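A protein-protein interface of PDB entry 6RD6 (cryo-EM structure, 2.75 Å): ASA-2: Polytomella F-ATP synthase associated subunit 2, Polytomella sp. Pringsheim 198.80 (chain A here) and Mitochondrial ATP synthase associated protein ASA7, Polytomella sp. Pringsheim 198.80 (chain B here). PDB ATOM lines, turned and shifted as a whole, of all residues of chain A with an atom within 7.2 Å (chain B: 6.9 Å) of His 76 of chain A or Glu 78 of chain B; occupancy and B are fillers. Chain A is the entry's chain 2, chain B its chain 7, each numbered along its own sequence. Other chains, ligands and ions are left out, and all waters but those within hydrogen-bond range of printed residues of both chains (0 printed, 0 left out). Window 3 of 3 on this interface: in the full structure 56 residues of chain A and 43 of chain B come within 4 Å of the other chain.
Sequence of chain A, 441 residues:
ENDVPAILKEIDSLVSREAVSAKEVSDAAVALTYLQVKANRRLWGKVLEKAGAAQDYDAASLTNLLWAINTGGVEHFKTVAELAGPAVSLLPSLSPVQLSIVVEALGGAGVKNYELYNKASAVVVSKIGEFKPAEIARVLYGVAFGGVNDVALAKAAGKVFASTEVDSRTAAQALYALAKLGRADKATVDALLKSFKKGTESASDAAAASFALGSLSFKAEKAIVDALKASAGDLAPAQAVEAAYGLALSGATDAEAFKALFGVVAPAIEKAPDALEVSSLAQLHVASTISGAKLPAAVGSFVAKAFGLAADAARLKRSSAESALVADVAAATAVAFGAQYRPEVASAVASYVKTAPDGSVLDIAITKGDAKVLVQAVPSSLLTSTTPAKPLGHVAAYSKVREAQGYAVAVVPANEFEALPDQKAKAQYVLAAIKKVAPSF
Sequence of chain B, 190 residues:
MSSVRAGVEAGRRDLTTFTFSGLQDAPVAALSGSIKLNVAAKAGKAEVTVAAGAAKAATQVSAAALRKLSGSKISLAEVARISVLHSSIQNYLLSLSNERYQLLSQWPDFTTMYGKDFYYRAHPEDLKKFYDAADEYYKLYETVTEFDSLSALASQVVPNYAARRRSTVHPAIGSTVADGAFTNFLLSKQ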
ATOM      1  N   LEU A  48      14.207  17.450  -8.917  1.00  0.00           N
ATOM      2  CA  LEU A  48      14.232  16.655  -7.691  1.00  0.00           C
ATOM      3  C   LEU A  48      12.870  16.640  -7.002  1.00  0.00           C
ATOM      4  O   LEU A  48      12.506  15.646  -6.365  1.00  0.00           O
ATOM      5  CB  LEU A  48      15.317  17.170  -6.745  1.00  0.00           C
ATOM      6  CG  LEU A  48      16.719  16.544  -6.779  1.00  0.00           C
ATOM      7  CD1 LEU A  48      16.676  15.121  -6.285  1.00  0.00           C
ATOM      8  CD2 LEU A  48      17.350  16.572  -8.146  1.00  0.00           C
ATOM      9  N   GLU A  49      12.088  17.713  -7.150  1.00  0.00           N
ATOM     10  CA  GLU A  49      10.717  17.714  -6.644  1.00  0.00           C
ATOM     11  C   GLU A  49       9.854  16.705  -7.386  1.00  0.00           C
ATOM     12  O   GLU A  49       9.092  15.950  -6.768  1.00  0.00           O
ATOM     13  CB  GLU A  49      10.111  19.106  -6.771  1.00  0.00           C
ATOM     14  CG  GLU A  49      10.467  20.052  -5.656  1.00  0.00           C
ATOM     15  CD  GLU A  49      10.292  21.495  -6.065  1.00  0.00           C
ATOM     16  OE1 GLU A  49       9.705  21.737  -7.137  1.00  0.00           O
ATOM     17  OE2 GLU A  49      10.743  22.386  -5.319  1.00  0.00           O
ATOM     18  N   ILE A  69      21.900  12.116 -10.400  1.00  0.00           N
ATOM     19  CA  ILE A  69      22.054  12.813  -9.129  1.00  0.00           C
ATOM     20  C   ILE A  69      23.480  12.674  -8.607  1.00  0.00           C
ATOM     21  O   ILE A  69      24.091  13.653  -8.160  1.00  0.00           O
ATOM     22  CB  ILE A  69      21.013  12.284  -8.121  1.00  0.00           C
ATOM     23  CG1 ILE A  69      19.629  12.827  -8.459  1.00  0.00           C
ATOM     24  CG2 ILE A  69      21.367  12.645  -6.695  1.00  0.00           C
ATOM     25  CD1 ILE A  69      18.528  12.154  -7.701  1.00  0.00           C
ATOM     26  N   GLY A  73      26.450  16.032  -9.036  1.00  0.00           N
ATOM     27  CA  GLY A  73      26.820  16.654  -7.786  1.00  0.00           C
ATOM     28  C   GLY A  73      25.668  17.276  -7.044  1.00  0.00           C
ATOM     29  O   GLY A  73      25.866  18.273  -6.344  1.00  0.00           O
ATOM     30  N   VAL A  74      24.470  16.723  -7.176  1.00  0.00           N
ATOM     31  CA  VAL A  74      23.269  17.316  -6.605  1.00  0.00           C
ATOM     32  C   VAL A  74      22.939  16.589  -5.310  1.00  0.00           C
ATOM     33  O   VAL A  74      22.654  15.389  -5.318  1.00  0.00           O
ATOM     34  CB  VAL A  74      22.099  17.241  -7.593  1.00  0.00           C
ATOM     35  CG1 VAL A  74      20.898  17.949  -7.031  1.00  0.00           C
ATOM     36  CG2 VAL A  74      22.509  17.850  -8.907  1.00  0.00           C
ATOM     37  N   GLU A  75      22.982  17.312  -4.198  1.00  0.00           N
ATOM     38  CA  GLU A  75      22.665  16.751  -2.894  1.00  0.00           C
ATOM     39  C   GLU A  75      21.373  17.353  -2.356  1.00  0.00           C
ATOM     40  O   GLU A  75      21.234  18.576  -2.253  1.00  0.00           O
ATOM     41  CB  GLU A  75      23.839  16.928  -1.919  1.00  0.00           C
ATOM     42  CG  GLU A  75      24.378  18.335  -1.739  1.00  0.00           C
ATOM     43  CD  GLU A  75      25.600  18.384  -0.840  1.00  0.00           C
ATOM     44  OE1 GLU A  75      26.010  17.320  -0.336  1.00  0.00           O
ATOM     45  OE2 GLU A  75      26.159  19.484  -0.652  1.00  0.00           O
ATOM     46  N   HIS A  76      20.405  16.482  -2.085  1.00  0.00           N
ATOM     47  CA  HIS A  76      19.191  16.828  -1.347  1.00  0.00           C
ATOM     48  C   HIS A  76      18.761  15.535  -0.662  1.00  0.00           C
ATOM     49  O   HIS A  76      18.213  14.644  -1.308  1.00  0.00           O
ATOM     50  CB  HIS A  76      18.092  17.381  -2.238  1.00  0.00           C
ATOM     51  CG  HIS A  76      16.842  17.732  -1.494  1.00  0.00           C
ATOM     52  ND1 HIS A  76      15.663  17.038  -1.655  1.00  0.00           N
ATOM     53  CD2 HIS A  76      16.591  18.693  -0.578  1.00  0.00           C
ATOM     54  CE1 HIS A  76      14.738  17.561  -0.871  1.00  0.00           C
ATOM     55  NE2 HIS A  76      15.276  18.568  -0.209  1.00  0.00           N
ATOM     56  N   PHE A  77      19.012  15.462   0.648  1.00  0.00           N
ATOM     57  CA  PHE A  77      18.980  14.185   1.354  1.00  0.00           C
ATOM     58  C   PHE A  77      17.579  13.597   1.426  1.00  0.00           C
ATOM     59  O   PHE A  77      17.421  12.373   1.464  1.00  0.00           O
ATOM     60  CB  PHE A  77      19.549  14.351   2.763  1.00  0.00           C
ATOM     61  CG  PHE A  77      19.548  13.087   3.562  1.00  0.00           C
ATOM     62  CD1 PHE A  77      20.435  12.069   3.265  1.00  0.00           C
ATOM     63  CD2 PHE A  77      18.644  12.901   4.589  1.00  0.00           C
ATOM     64  CE1 PHE A  77      20.427  10.900   3.988  1.00  0.00           C
ATOM     65  CE2 PHE A  77      18.633  11.732   5.315  1.00  0.00           C
ATOM     66  CZ  PHE A  77      19.526  10.733   5.014  1.00  0.00           C
ATOM     67  N   LYS A  78      16.552  14.447   1.416  1.00  0.00           N
ATOM     68  CA  LYS A  78      15.184  13.963   1.564  1.00  0.00           C
ATOM     69  C   LYS A  78      14.742  13.161   0.347  1.00  0.00           C
ATOM     70  O   LYS A  78      14.251  12.035   0.481  1.00  0.00           O
ATOM     71  CB  LYS A  78      14.239  15.133   1.809  1.00  0.00           C
ATOM     72  CG  LYS A  78      12.780  14.744   1.808  1.00  0.00           C
ATOM     73  CD  LYS A  78      11.952  15.747   2.568  1.00  0.00           C
ATOM     74  CE  LYS A  78      10.553  15.819   2.008  1.00  0.00           C
ATOM     75  NZ  LYS A  78      10.008  14.466   1.743  1.00  0.00           N
ATOM     76  N   THR A  79      14.956  13.706  -0.852  1.00  0.00           N
ATOM     77  CA  THR A  79      14.521  13.033  -2.072  1.00  0.00           C
ATOM     78  C   THR A  79      15.330  11.769  -2.329  1.00  0.00           C
ATOM     79  O   THR A  79      14.764  10.709  -2.619  1.00  0.00           O
ATOM     80  CB  THR A  79      14.632  13.973  -3.267  1.00  0.00           C
ATOM     81  OG1 THR A  79      14.000  15.221  -2.960  1.00  0.00           O
ATOM     82  CG2 THR A  79      13.950  13.354  -4.467  1.00  0.00           C
ATOM     83  N   VAL A  80      16.653  11.862  -2.206  1.00  0.00           N
ATOM     84  CA  VAL A  80      17.517  10.715  -2.461  1.00  0.00           C
ATOM     85  C   VAL A  80      17.313   9.636  -1.403  1.00  0.00           C
ATOM     86  O   VAL A  80      17.348   8.441  -1.704  1.00  0.00           O
ATOM     87  CB  VAL A  80      18.982  11.176  -2.545  1.00  0.00           C
ATOM     88  CG1 VAL A  80      19.857  10.069  -3.042  1.00  0.00           C
ATOM     89  CG2 VAL A  80      19.098  12.351  -3.486  1.00  0.00           C
ATOM     90  N   ALA A  81      17.035  10.033  -0.162  1.00  0.00           N
ATOM     91  CA  ALA A  81      16.842   9.044   0.890  1.00  0.00           C
ATOM     92  C   ALA A  81      15.450   8.432   0.837  1.00  0.00           C
ATOM     93  O   ALA A  81      15.228   7.336   1.362  1.00  0.00           O
ATOM     94  CB  ALA A  81      17.112   9.675   2.252  1.00  0.00           C
ATOM     95  N   GLU A  82      14.493   9.121   0.211  1.00  0.00           N
ATOM     96  CA  GLU A  82      13.189   8.506  -0.003  1.00  0.00           C
ATOM     97  C   GLU A  82      13.161   7.719  -1.306  1.00  0.00           C
ATOM     98  O   GLU A  82      12.219   6.960  -1.561  1.00  0.00           O
ATOM     99  CB  GLU A  82      12.096   9.568   0.018  1.00  0.00           C
ATOM    100  CG  GLU A  82      11.728  10.015   1.417  1.00  0.00           C
ATOM    101  CD  GLU A  82      10.889  11.264   1.424  1.00  0.00           C
ATOM    102  OE1 GLU A  82      10.821  11.935   0.376  1.00  0.00           O
ATOM    103  OE2 GLU A  82      10.300  11.578   2.477  1.00  0.00           O
ATOM    104  N   LEU A  83      14.189   7.879  -2.139  1.00  0.00           N
ATOM    105  CA  LEU A  83      14.375   7.001  -3.292  1.00  0.00           C
ATOM    106  C   LEU A  83      14.919   5.628  -2.916  1.00  0.00           C
ATOM    107  O   LEU A  83      15.117   4.800  -3.809  1.00  0.00           O
ATOM    108  CB  LEU A  83      15.327   7.634  -4.301  1.00  0.00           C
ATOM    109  CG  LEU A  83      14.805   8.713  -5.240  1.00  0.00           C
ATOM    110  CD1 LEU A  83      15.965   9.556  -5.702  1.00  0.00           C
ATOM    111  CD2 LEU A  83      14.083   8.104  -6.411  1.00  0.00           C
ATOM    112  N   ALA A 109      25.295   9.633  -1.093  1.00  0.00           N
ATOM    113  CA  ALA A 109      24.407  10.663  -0.572  1.00  0.00           C
ATOM    114  C   ALA A 109      24.292  10.602   0.944  1.00  0.00           C
ATOM    115  O   ALA A 109      23.896  11.587   1.574  1.00  0.00           O
ATOM    116  CB  ALA A 109      23.029  10.534  -1.207  1.00  0.00           C
ATOM    117  N   LEU B  15      26.549  14.669  -0.096  1.00  0.00           N
ATOM    118  CA  LEU B  15      27.403  13.968  -1.044  1.00  0.00           C
ATOM    119  C   LEU B  15      28.863  14.060  -0.611  1.00  0.00           C
ATOM    120  O   LEU B  15      29.275  15.043  -0.002  1.00  0.00           O
ATOM    121  CB  LEU B  15      27.212  14.536  -2.452  1.00  0.00           C
ATOM    122  CG  LEU B  15      27.596  13.657  -3.645  1.00  0.00           C
ATOM    123  CD1 LEU B  15      27.128  12.230  -3.460  1.00  0.00           C
ATOM    124  CD2 LEU B  15      27.033  14.232  -4.928  1.00  0.00           C
ATOM    125  N   ILE B  74      25.713  21.063  -5.626  1.00  0.00           N
ATOM    126  CA  ILE B  74      24.462  21.804  -5.573  1.00  0.00           C
ATOM    127  C   ILE B  74      23.693  21.303  -4.362  1.00  0.00           C
ATOM    128  O   ILE B  74      23.134  20.200  -4.385  1.00  0.00           O
ATOM    129  CB  ILE B  74      23.639  21.630  -6.858  1.00  0.00           C
ATOM    130  CG1 ILE B  74      24.414  22.145  -8.065  1.00  0.00           C
ATOM    131  CG2 ILE B  74      22.321  22.370  -6.749  1.00  0.00           C
ATOM    132  CD1 ILE B  74      23.710  21.907  -9.372  1.00  0.00           C
ATOM    133  N   SER B  75      23.685  22.092  -3.297  1.00  0.00           N
ATOM    134  CA  SER B  75      22.924  21.774  -2.101  1.00  0.00           C
ATOM    135  C   SER B  75      21.519  22.332  -2.266  1.00  0.00           C
ATOM    136  O   SER B  75      21.278  23.512  -1.993  1.00  0.00           O
ATOM    137  CB  SER B  75      23.592  22.345  -0.854  1.00  0.00           C
ATOM    138  OG  SER B  75      24.845  21.727  -0.628  1.00  0.00           O
ATOM    139  N   LEU B  76      20.601  21.490  -2.724  1.00  0.00           N
ATOM    140  CA  LEU B  76      19.221  21.891  -2.934  1.00  0.00           C
ATOM    141  C   LEU B  76      18.541  22.013  -1.580  1.00  0.00           C
ATOM    142  O   LEU B  76      18.629  21.103  -0.751  1.00  0.00           O
ATOM    143  CB  LEU B  76      18.492  20.887  -3.822  1.00  0.00           C
ATOM    144  CG  LEU B  76      18.831  20.968  -5.304  1.00  0.00           C
ATOM    145  CD1 LEU B  76      17.959  20.013  -6.064  1.00  0.00           C
ATOM    146  CD2 LEU B  76      18.644  22.377  -5.820  1.00  0.00           C
ATOM    147  N   ALA B  77      17.879  23.139  -1.352  1.00  0.00           N
ATOM    148  CA  ALA B  77      17.266  23.433  -0.068  1.00  0.00           C
ATOM    149  C   ALA B  77      15.889  24.030  -0.296  1.00  0.00           C
ATOM    150  O   ALA B  77      15.687  24.784  -1.252  1.00  0.00           O
ATOM    151  CB  ALA B  77      18.140  24.382   0.742  1.00  0.00           C
ATOM    152  N   GLU B  78      14.952  23.694   0.581  1.00  0.00           N
ATOM    153  CA  GLU B  78      13.581  24.150   0.434  1.00  0.00           C
ATOM    154  C   GLU B  78      13.449  25.607   0.853  1.00  0.00           C
ATOM    155  O   GLU B  78      14.022  26.036   1.856  1.00  0.00           O
ATOM    156  CB  GLU B  78      12.646  23.280   1.271  1.00  0.00           C
ATOM    157  CG  GLU B  78      12.618  21.816   0.871  1.00  0.00           C
ATOM    158  CD  GLU B  78      13.620  20.972   1.636  1.00  0.00           C
ATOM    159  OE1 GLU B  78      14.459  21.546   2.360  1.00  0.00           O
ATOM    160  OE2 GLU B  78      13.567  19.732   1.525  1.00  0.00           O
ATOM    161  N   VAL B  79      12.696  26.370   0.069  1.00  0.00           N
ATOM    162  CA  VAL B  79      12.313  27.728   0.434  1.00  0.00           C
ATOM    163  C   VAL B  79      10.884  27.661   0.951  1.00  0.00           C
ATOM    164  O   VAL B  79       9.930  27.642   0.172  1.00  0.00           O
ATOM    165  CB  VAL B  79      12.433  28.691  -0.751  1.00  0.00           C
ATOM    166  CG1 VAL B  79      12.126  30.106  -0.315  1.00  0.00           C
ATOM    167  CG2 VAL B  79      13.813  28.610  -1.349  1.00  0.00           C
ATOM    168  N   ALA B  80      10.734  27.610   2.267  1.00  0.00           N
ATOM    169  CA  ALA B  80       9.440  27.427   2.899  1.00  0.00           C
ATOM    170  C   ALA B  80       8.922  28.758   3.414  1.00  0.00           C
ATOM    171  O   ALA B  80       9.701  29.681   3.665  1.00  0.00           O
ATOM    172  CB  ALA B  80       9.529  26.424   4.043  1.00  0.00           C
ATOM    173  N   VAL B  84      10.006  23.785   6.908  1.00  0.00           N
ATOM    174  CA  VAL B  84       9.729  22.534   6.213  1.00  0.00           C
ATOM    175  C   VAL B  84       8.812  21.658   7.057  1.00  0.00           C
ATOM    176  O   VAL B  84       7.934  20.958   6.535  1.00  0.00           O
ATOM    177  CB  VAL B  84      11.058  21.832   5.876  1.00  0.00           C
ATOM    178  CG1 VAL B  84      10.834  20.627   5.022  1.00  0.00           C
ATOM    179  CG2 VAL B  84      11.983  22.795   5.175  1.00  0.00           C
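The backbone NH (N) of Ile 74 of chain B sits at hydrogen-bond distance from the backbone carbonyl oxygen (O) of Gly 73 of chain A. The side-chain carboxylate (OE2) of Glu 75 of chain A sits at hydrogen-bond distance from the side-chain hydroxyl (OG) of Ser 75 of chain B, at 2.6 Å. The side-chain carboxylate (OE1) of Glu 75 of chain A is in hydrogen-bond range of the backbone NH (N) of Leu 15 of chain B (2.7 Å). N of Glu 75 of chain A lies within hydrogen-bond range of O of Ile 74 of chain B, at 2.9 Å. The backbone carbonyl oxygen (O) of Glu 75 of chain A lies within hydrogen-bond range of the backbone NH (N) of Leu 76 of chain B (3.0 Å). A ring nitrogen (NE2) of His 76 of chain A is in hydrogen-bond range of the side-chain carboxylate (OE2) of Glu 78 of chain B (2.7 Å).
The backbone carbonyl oxygen of Ile 69 of chain A is in hydrogen-bond range of the backbone NH of Val 74 of chain A (3.2 Å). A ring nitrogen (ND1) of His 76 of chain A sits at hydrogen-bond distance from the side-chain hydroxyl (OG1) of Thr 79 of chain A (2.8 Å).
Among the printed residues, pairs that only touch across the chains: Leu 48 of chain A with Leu 76 of chain B, Gly 73 of chain A with Leu 15 of chain B, Val 74 of chain A with Ile 74 of chain B, Val 74 of chain A with Leu 76 of chain B, His 76 of chain A with Leu 76 of chain B and Ala 109 of chain A with Leu 15 of chain B.
Of the printed residues of chain B, Gly 73 of chain A touches Leu 15 and Ile 74. Of chain B, only Leu 76 and Glu 78 come within 4 Å of His 76 of chain A. Lys 78 of chain A touches none of the printed residues of chain B. Thr 79 of chain A touches none of the printed residues of chain B. Of the printed residues of chain A, Leu 15 of chain B touches Gly 73, Glu 75 and Ala 109. Of the printed residues of chain A, Ile 74 of chain B touches Gly 73, Val 74 and Glu 75. Of the printed residues of chain A, Ser 75 of chain B touches Glu 75 (2.6 Å). Of the printed residues of chain A, Leu 76 of chain B touches Leu 48, Val 74, Glu 75 and His 76. Printed residues of chain A within 4 Å of Glu 78 of chain B: His 76 (2.7 Å). The nearest residue of chain B that does not touch His 76 of chain A is Ala 77 of chain B (4.7 Å). The nearest residue of chain A that does not touch Glu 78 of chain B is Lys 78 of chain A (4.4 Å).
Of the 9 printed residues of chain B, 5 touch a printed residue of chain A. Printed residues of chain B that touch a printed residue of chain A: Leu 15, Ile 74, Ser 75, Leu 76 and Glu 78. Of the 15 printed residues of chain A, 6 touch a printed residue of chain B. Hydrophobic or aromatic side chains of chain A that line the printed part of chain B: Leu 48, Val 74 and His 76. Along chain A the printed residues that touch a printed residue of chain B span positions 48 to 109. Among the printed residues, 12 pairs touch across the chains. Among the printed residues, no Asp or Glu carboxylate lies within 4 Å of a Lys or Arg side-chain nitrogen of the other chain.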
